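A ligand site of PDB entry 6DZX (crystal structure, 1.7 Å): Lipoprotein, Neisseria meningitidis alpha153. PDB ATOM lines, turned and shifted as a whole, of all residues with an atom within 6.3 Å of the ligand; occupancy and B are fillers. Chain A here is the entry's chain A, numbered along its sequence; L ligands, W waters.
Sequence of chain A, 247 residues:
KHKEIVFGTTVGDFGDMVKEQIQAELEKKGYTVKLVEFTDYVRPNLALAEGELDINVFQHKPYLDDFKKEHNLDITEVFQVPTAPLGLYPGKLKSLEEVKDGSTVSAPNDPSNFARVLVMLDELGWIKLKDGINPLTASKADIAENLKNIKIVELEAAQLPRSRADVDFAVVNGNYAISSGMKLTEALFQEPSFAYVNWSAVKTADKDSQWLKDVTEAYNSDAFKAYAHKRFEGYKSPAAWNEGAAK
The side-chain amide oxygen (OD1) of Asn 198 sits at hydrogen-bond distance from a nitrogen (N1) of the ligand (2.7 Å). ND2 of Asn 173 sits at hydrogen-bond distance from O1 of the ligand (3.0 Å). The guanidinium group (NH1) of Arg 116 lies within salt-bridge range of an oxygen (O1) of the ligand (3.1 Å). O of Phe 58 is in hydrogen-bond range of N1 of the ligand, 3.3 Å away. NE2 of His 60 sits close to S1 of the ligand (3.4 Å). S1 of the ligand sits close to ND2 of Asn 113 (3.6 Å).
N of Gln 59 is in hydrogen-bond range of OD1 of Asn 198 (3.4 Å). OD1 of Asn 113 sits at hydrogen-bond distance from ND2 of Asn 173 (3.3 Å). The guanidinium group (NH1) of Arg 116 sits close to a ring nitrogen (NE2) of His 60 (3.4 Å). OD1 of Asn 113 lies within hydrogen-bond range of NH1 of Arg 116 (3.0 Å). The side-chain hydroxyl of Tyr 63 sits at hydrogen-bond distance from the backbone carbonyl oxygen of Tyr 41. OD1 of Asn 113 is in hydrogen-bond range of NE2 of His 60 (2.9 Å). A ring nitrogen (ND1) of His 60 lies within hydrogen-bond range of the backbone NH (N) of Tyr 63. The side-chain carboxylate (OD2) of Asp 110 lies within hydrogen-bond range of the side-chain amide nitrogen (ND2) of Asn 113 (2.7 Å).
Residues that only touch the ligand: Phe 14, Tyr 41, Gln 59, Tyr 63, Thr 83, Asn 175 and Tyr 196. Within 4 Å of the ligand: Phe 14, Tyr 41, Phe 58, Gln 59, His 60, Tyr 63, Thr 83, Asn 113, Arg 116, Asn 173, Asn 175, Tyr 196 and Asn 198.
Water W4 lies within hydrogen-bond range of an oxygen (O2) of the ligand (2.7 Å), the backbone carbonyl oxygen of Ala 84 (2.9 Å) and the guanidinium group of Arg 116 (2.9 Å). Water W3 lies within hydrogen-bond range of O1 of the ligand (2.7 Å), N of Gly 174 (2.9 Å), N of Leu 86 (3.2 Å) and O of Ala 84 (3.5 Å). Water W1 lies within hydrogen-bond range of the backbone carbonyl oxygen of Phe 58, the side-chain hydroxyl of Thr 10, a nitrogen (N1) of the ligand and the side-chain amide oxygen of Asn 175. Water W2 lies within hydrogen-bond range of a nitrogen (N1) of the ligand (3.0 Å), the backbone NH (N) of Asn 175 (3.0 Å) and the backbone carbonyl oxygen (O) of Ala 84 (3.1 Å).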
ATOM      1  N   THR A  10      -8.041 -18.648  -3.237  1.00  0.00           N
ATOM      2  CA  THR A  10      -8.584 -19.869  -2.683  1.00  0.00           C
ATOM      3  C   THR A  10     -10.023 -19.627  -2.178  1.00  0.00           C
ATOM      4  O   THR A  10     -10.450 -18.485  -2.016  1.00  0.00           O
ATOM      5  CB  THR A  10      -7.675 -20.393  -1.550  1.00  0.00           C
ATOM      6  OG1 THR A  10      -7.148 -19.298  -0.800  1.00  0.00           O
ATOM      7  CG2 THR A  10      -6.543 -21.162  -2.145  1.00  0.00           C
ATOM      8  N   PHE A  14     -10.302 -15.242   1.306  1.00  0.00           N
ATOM      9  CA  PHE A  14      -9.780 -14.297   0.308  1.00  0.00           C
ATOM     10  C   PHE A  14     -10.803 -13.964  -0.793  1.00  0.00           C
ATOM     11  O   PHE A  14     -10.768 -12.854  -1.339  1.00  0.00           O
ATOM     12  CB  PHE A  14      -8.495 -14.857  -0.328  1.00  0.00           C
ATOM     13  CG  PHE A  14      -7.292 -14.907   0.609  1.00  0.00           C
ATOM     14  CD1 PHE A  14      -7.013 -13.868   1.475  1.00  0.00           C
ATOM     15  CD2 PHE A  14      -6.420 -15.998   0.578  1.00  0.00           C
ATOM     16  CE1 PHE A  14      -5.929 -13.896   2.313  1.00  0.00           C
ATOM     17  CE2 PHE A  14      -5.326 -16.041   1.418  1.00  0.00           C
ATOM     18  CZ  PHE A  14      -5.061 -14.975   2.288  1.00  0.00           C
ATOM     19  N   TYR A  41      -3.276 -25.165  -4.265  1.00  0.00           N
ATOM     20  CA  TYR A  41      -2.228 -24.157  -4.289  1.00  0.00           C
ATOM     21  C   TYR A  41      -1.404 -24.159  -5.588  1.00  0.00           C
ATOM     22  O   TYR A  41      -0.504 -23.333  -5.751  1.00  0.00           O
ATOM     23  CB  TYR A  41      -1.284 -24.352  -3.103  1.00  0.00           C
ATOM     24  CG  TYR A  41      -1.844 -24.115  -1.729  1.00  0.00           C
ATOM     25  CD1 TYR A  41      -2.937 -23.301  -1.468  1.00  0.00           C
ATOM     26  CD2 TYR A  41      -1.195 -24.704  -0.646  1.00  0.00           C
ATOM     27  CE1 TYR A  41      -3.361 -23.073  -0.137  1.00  0.00           C
ATOM     28  CE2 TYR A  41      -1.581 -24.480   0.634  1.00  0.00           C
ATOM     29  CZ  TYR A  41      -2.664 -23.701   0.891  1.00  0.00           C
ATOM     30  OH  TYR A  41      -2.994 -23.551   2.213  1.00  0.00           O
ATOM     31  N   PHE A  58      -3.579 -15.678  -2.755  1.00  0.00           N
ATOM     32  CA  PHE A  58      -3.708 -16.932  -2.019  1.00  0.00           C
ATOM     33  C   PHE A  58      -2.466 -17.415  -1.297  1.00  0.00           C
ATOM     34  O   PHE A  58      -2.529 -18.439  -0.624  1.00  0.00           O
ATOM     35  CB  PHE A  58      -4.166 -18.045  -2.979  1.00  0.00           C
ATOM     36  CG  PHE A  58      -3.025 -18.628  -3.794  1.00  0.00           C
ATOM     37  CD1 PHE A  58      -2.500 -17.952  -4.894  1.00  0.00           C
ATOM     38  CD2 PHE A  58      -2.465 -19.844  -3.448  1.00  0.00           C
ATOM     39  CE1 PHE A  58      -1.462 -18.463  -5.585  1.00  0.00           C
ATOM     40  CE2 PHE A  58      -1.433 -20.354  -4.148  1.00  0.00           C
ATOM     41  CZ  PHE A  58      -0.929 -19.680  -5.223  1.00  0.00           C
ATOM     42  N   GLN A  59      -1.301 -16.751  -1.478  1.00  0.00           N
ATOM     43  CA  GLN A  59      -0.018 -17.350  -1.129  1.00  0.00           C
ATOM     44  C   GLN A  59       0.842 -16.357  -0.356  1.00  0.00           C
ATOM     45  O   GLN A  59       0.656 -15.137  -0.435  1.00  0.00           O
ATOM     46  CB  GLN A  59       0.699 -17.793  -2.399  1.00  0.00           C
ATOM     47  CG  GLN A  59       1.325 -16.669  -3.106  1.00  0.00           C
ATOM     48  CD  GLN A  59       1.605 -16.984  -4.568  1.00  0.00           C
ATOM     49  OE1 GLN A  59       2.340 -17.944  -4.881  1.00  0.00           O
ATOM     50  NE2 GLN A  59       0.995 -16.216  -5.464  1.00  0.00           N
ATOM     51  N   HIS A  60       1.822 -16.892   0.358  1.00  0.00           N
ATOM     52  CA  HIS A  60       2.866 -16.066   0.957  1.00  0.00           C
ATOM     53  C   HIS A  60       4.075 -16.026   0.023  1.00  0.00           C
ATOM     54  O   HIS A  60       4.146 -16.759  -0.969  1.00  0.00           O
ATOM     55  CB  HIS A  60       3.230 -16.566   2.362  1.00  0.00           C
ATOM     56  CG  HIS A  60       3.457 -18.036   2.465  1.00  0.00           C
ATOM     57  ND1 HIS A  60       4.540 -18.680   1.883  1.00  0.00           N
ATOM     58  CD2 HIS A  60       2.768 -18.998   3.130  1.00  0.00           C
ATOM     59  CE1 HIS A  60       4.483 -19.967   2.159  1.00  0.00           C
ATOM     60  NE2 HIS A  60       3.417 -20.180   2.920  1.00  0.00           N
ATOM     61  N   TYR A  63       6.361 -19.154  -0.598  1.00  0.00           N
ATOM     62  CA  TYR A  63       5.721 -20.039  -1.567  1.00  0.00           C
ATOM     63  C   TYR A  63       5.890 -19.491  -2.986  1.00  0.00           C
ATOM     64  O   TYR A  63       6.354 -20.198  -3.904  1.00  0.00           O
ATOM     65  CB  TYR A  63       4.238 -20.210  -1.240  1.00  0.00           C
ATOM     66  CG  TYR A  63       3.556 -21.227  -2.113  1.00  0.00           C
ATOM     67  CD1 TYR A  63       3.017 -20.884  -3.376  1.00  0.00           C
ATOM     68  CD2 TYR A  63       3.462 -22.531  -1.720  1.00  0.00           C
ATOM     69  CE1 TYR A  63       2.399 -21.860  -4.185  1.00  0.00           C
ATOM     70  CE2 TYR A  63       2.866 -23.483  -2.512  1.00  0.00           C
ATOM     71  CZ  TYR A  63       2.351 -23.159  -3.734  1.00  0.00           C
ATOM     72  OH  TYR A  63       1.785 -24.175  -4.489  1.00  0.00           O
ATOM     73  N   THR A  83      -4.261 -12.067   6.689  1.00  0.00           N
ATOM     74  CA  THR A  83      -3.977 -13.486   6.497  1.00  0.00           C
ATOM     75  C   THR A  83      -4.317 -14.304   7.721  1.00  0.00           C
ATOM     76  O   THR A  83      -3.916 -13.968   8.843  1.00  0.00           O
ATOM     77  CB  THR A  83      -2.511 -13.662   6.149  1.00  0.00           C
ATOM     78  OG1 THR A  83      -2.230 -12.971   4.909  1.00  0.00           O
ATOM     79  CG2 THR A  83      -2.150 -15.141   6.001  1.00  0.00           C
ATOM     80  N   ALA A  84      -5.044 -15.413   7.493  1.00  0.00           N
ATOM     81  CA  ALA A  84      -5.338 -16.367   8.570  1.00  0.00           C
ATOM     82  C   ALA A  84      -4.048 -17.086   8.972  1.00  0.00           C
ATOM     83  O   ALA A  84      -3.353 -17.654   8.116  1.00  0.00           O
ATOM     84  CB  ALA A  84      -6.403 -17.375   8.139  1.00  0.00           C
ATOM     85  N   PRO A  85      -3.691 -17.083  10.254  1.00  0.00           N
ATOM     86  CA  PRO A  85      -2.400 -17.664  10.639  1.00  0.00           C
ATOM     87  C   PRO A  85      -2.394 -19.181  10.597  1.00  0.00           C
ATOM     88  O   PRO A  85      -3.427 -19.864  10.650  1.00  0.00           O
ATOM     89  CB  PRO A  85      -2.195 -17.166  12.078  1.00  0.00           C
ATOM     90  CG  PRO A  85      -3.550 -16.870  12.563  1.00  0.00           C
ATOM     91  CD  PRO A  85      -4.372 -16.443  11.387  1.00  0.00           C
ATOM     92  N   LEU A  86      -1.166 -19.722  10.568  1.00  0.00           N
ATOM     93  CA  LEU A  86      -0.929 -21.152  10.699  1.00  0.00           C
ATOM     94  C   LEU A  86      -1.056 -21.566  12.158  1.00  0.00           C
ATOM     95  O   LEU A  86      -0.564 -20.872  13.046  1.00  0.00           O
ATOM     96  CB  LEU A  86       0.475 -21.477  10.223  1.00  0.00           C
ATOM     97  CG  LEU A  86       0.871 -22.969  10.111  1.00  0.00           C
ATOM     98  CD1 LEU A  86       0.144 -23.675   8.972  1.00  0.00           C
ATOM     99  CD2 LEU A  86       2.347 -23.114   9.935  1.00  0.00           C
ATOM    100  N   ASP A 110       4.293 -29.430   0.714  1.00  0.00           N
ATOM    101  CA  ASP A 110       5.069 -28.567  -0.166  1.00  0.00           C
ATOM    102  C   ASP A 110       6.172 -27.888   0.653  1.00  0.00           C
ATOM    103  O   ASP A 110       6.001 -27.659   1.851  1.00  0.00           O
ATOM    104  CB  ASP A 110       4.170 -27.539  -0.831  1.00  0.00           C
ATOM    105  CG  ASP A 110       3.512 -26.610   0.170  1.00  0.00           C
ATOM    106  OD1 ASP A 110       2.556 -27.035   0.870  1.00  0.00           O
ATOM    107  OD2 ASP A 110       4.038 -25.501   0.324  1.00  0.00           O
ATOM    108  N   SER A 112       7.848 -24.898   1.153  1.00  0.00           N
ATOM    109  CA  SER A 112       7.847 -23.639   1.903  1.00  0.00           C
ATOM    110  C   SER A 112       6.899 -23.699   3.087  1.00  0.00           C
ATOM    111  O   SER A 112       7.165 -23.069   4.123  1.00  0.00           O
ATOM    112  CB  SER A 112       7.476 -22.458   0.994  1.00  0.00           C
ATOM    113  OG  SER A 112       6.103 -22.476   0.645  1.00  0.00           O
ATOM    114  N   ASN A 113       5.808 -24.437   2.969  1.00  0.00           N
ATOM    115  CA  ASN A 113       4.907 -24.621   4.105  1.00  0.00           C
ATOM    116  C   ASN A 113       5.386 -25.714   5.060  1.00  0.00           C
ATOM    117  O   ASN A 113       5.186 -25.602   6.263  1.00  0.00           O
ATOM    118  CB  ASN A 113       3.513 -24.932   3.616  1.00  0.00           C
ATOM    119  CG  ASN A 113       2.849 -23.690   3.052  1.00  0.00           C
ATOM    120  OD1 ASN A 113       2.561 -22.752   3.809  1.00  0.00           O
ATOM    121  ND2 ASN A 113       2.678 -23.645   1.731  1.00  0.00           N
ATOM    122  N   ARG A 116       7.628 -24.259   7.702  1.00  0.00           N
ATOM    123  CA  ARG A 116       6.906 -23.625   8.800  1.00  0.00           C
ATOM    124  C   ARG A 116       6.615 -24.611   9.915  1.00  0.00           C
ATOM    125  O   ARG A 116       6.660 -24.260  11.095  1.00  0.00           O
ATOM    126  CB  ARG A 116       5.586 -23.057   8.296  1.00  0.00           C
ATOM    127  CG  ARG A 116       5.794 -22.039   7.194  1.00  0.00           C
ATOM    128  CD  ARG A 116       4.473 -21.632   6.580  1.00  0.00           C
ATOM    129  NE  ARG A 116       3.711 -20.699   7.407  1.00  0.00           N
ATOM    130  CZ  ARG A 116       2.506 -20.267   7.089  1.00  0.00           C
ATOM    131  NH1 ARG A 116       1.937 -20.743   5.972  1.00  0.00           N
ATOM    132  NH2 ARG A 116       1.886 -19.354   7.853  1.00  0.00           N
ATOM    133  N   ASN A 173      -3.092 -24.980   7.436  1.00  0.00           N
ATOM    134  CA  ASN A 173      -3.051 -23.627   6.880  1.00  0.00           C
ATOM    135  C   ASN A 173      -4.344 -22.877   7.185  1.00  0.00           C
ATOM    136  O   ASN A 173      -5.446 -23.430   7.082  1.00  0.00           O
ATOM    137  CB  ASN A 173      -2.851 -23.711   5.353  1.00  0.00           C
ATOM    138  CG  ASN A 173      -1.492 -24.284   4.959  1.00  0.00           C
ATOM    139  OD1 ASN A 173      -1.346 -25.493   4.774  1.00  0.00           O
ATOM    140  ND2 ASN A 173      -0.488 -23.410   4.824  1.00  0.00           N
ATOM    141  N   GLY A 174      -4.206 -21.601   7.503  1.00  0.00           N
ATOM    142  CA  GLY A 174      -5.357 -20.827   7.915  1.00  0.00           C
ATOM    143  C   GLY A 174      -6.511 -20.850   6.941  1.00  0.00           C
ATOM    144  O   GLY A 174      -7.671 -21.001   7.339  1.00  0.00           O
ATOM    145  N   ASN A 175      -6.240 -20.722   5.626  1.00  0.00           N
ATOM    146  CA  ASN A 175      -7.345 -20.678   4.683  1.00  0.00           C
ATOM    147  C   ASN A 175      -8.171 -21.960   4.739  1.00  0.00           C
ATOM    148  O   ASN A 175      -9.404 -21.909   4.644  1.00  0.00           O
ATOM    149  CB  ASN A 175      -6.842 -20.435   3.252  1.00  0.00           C
ATOM    150  CG  ASN A 175      -6.052 -21.610   2.705  1.00  0.00           C
ATOM    151  OD1 ASN A 175      -4.925 -21.862   3.142  1.00  0.00           O
ATOM    152  ND2 ASN A 175      -6.635 -22.335   1.748  1.00  0.00           N
ATOM    153  N   TYR A 196       4.857 -14.818   6.758  1.00  0.00           N
ATOM    154  CA  TYR A 196       3.932 -15.532   5.898  1.00  0.00           C
ATOM    155  C   TYR A 196       2.600 -14.795   5.675  1.00  0.00           C
ATOM    156  O   TYR A 196       1.635 -15.393   5.187  1.00  0.00           O
ATOM    157  CB  TYR A 196       3.728 -16.931   6.453  1.00  0.00           C
ATOM    158  CG  TYR A 196       5.037 -17.726   6.433  1.00  0.00           C
ATOM    159  CD1 TYR A 196       5.502 -18.352   5.252  1.00  0.00           C
ATOM    160  CD2 TYR A 196       5.811 -17.806   7.564  1.00  0.00           C
ATOM    161  CE1 TYR A 196       6.680 -19.077   5.250  1.00  0.00           C
ATOM    162  CE2 TYR A 196       6.989 -18.509   7.567  1.00  0.00           C
ATOM    163  CZ  TYR A 196       7.440 -19.119   6.411  1.00  0.00           C
ATOM    164  OH  TYR A 196       8.627 -19.825   6.480  1.00  0.00           O
ATOM    165  N   VAL A 197       2.535 -13.508   5.996  1.00  0.00           N
ATOM    166  CA  VAL A 197       1.402 -12.699   5.583  1.00  0.00           C
ATOM    167  C   VAL A 197       1.328 -12.692   4.065  1.00  0.00           C
ATOM    168  O   VAL A 197       2.338 -12.435   3.400  1.00  0.00           O
ATOM    169  CB  VAL A 197       1.547 -11.294   6.159  1.00  0.00           C
ATOM    170  CG1 VAL A 197       0.427 -10.385   5.626  1.00  0.00           C
ATOM    171  CG2 VAL A 197       1.480 -11.355   7.710  1.00  0.00           C
ATOM    172  N   ASN A 198       0.164 -13.003   3.533  1.00  0.00           N
ATOM    173  CA  ASN A 198       0.065 -13.327   2.113  1.00  0.00           C
ATOM    174  C   ASN A 198       0.139 -12.075   1.254  1.00  0.00           C
ATOM    175  O   ASN A 198      -0.124 -10.948   1.707  1.00  0.00           O
ATOM    176  CB  ASN A 198      -1.236 -14.064   1.806  1.00  0.00           C
ATOM    177  CG  ASN A 198      -1.247 -15.516   2.244  1.00  0.00           C
ATOM    178  OD1 ASN A 198      -2.108 -16.291   1.792  1.00  0.00           O
ATOM    179  ND2 ASN A 198      -0.293 -15.922   3.117  1.00  0.00           N
HETATM  180  N1  LIG L   1      -2.707 -18.744   2.684  1.00  0.00           N
HETATM  181  C1  LIG L   1      -1.375 -19.334   2.696  1.00  0.00           C
HETATM  182  C2  LIG L   1      -0.910 -19.413   4.144  1.00  0.00           C
HETATM  183  O1  LIG L   1      -0.886 -20.479   4.798  1.00  0.00           O
HETATM  184  C3  LIG L   1      -1.389 -20.661   1.978  1.00  0.00           C
HETATM  185  C4  LIG L   1       0.026 -21.252   1.824  1.00  0.00           C
HETATM  186  S1  LIG L   1       1.041 -20.643   0.503  1.00  0.00           S
HETATM  187  C5  LIG L   1       0.096 -21.218  -0.851  1.00  0.00           C
HETATM  188  O2  LIG L   1      -0.518 -18.335   4.638  1.00  0.00           O
HETATM  189  O   HOH W   1      -4.597 -19.618   0.580  1.00  0.00           O
HETATM  190  O   HOH W   2      -4.114 -18.572   5.308  1.00  0.00           O
HETATM  191  O   HOH W   3      -1.546 -20.562   7.463  1.00  0.00           O
HETATM  192  O   HOH W   4      -0.581 -17.861   7.292  1.00  0.00           O
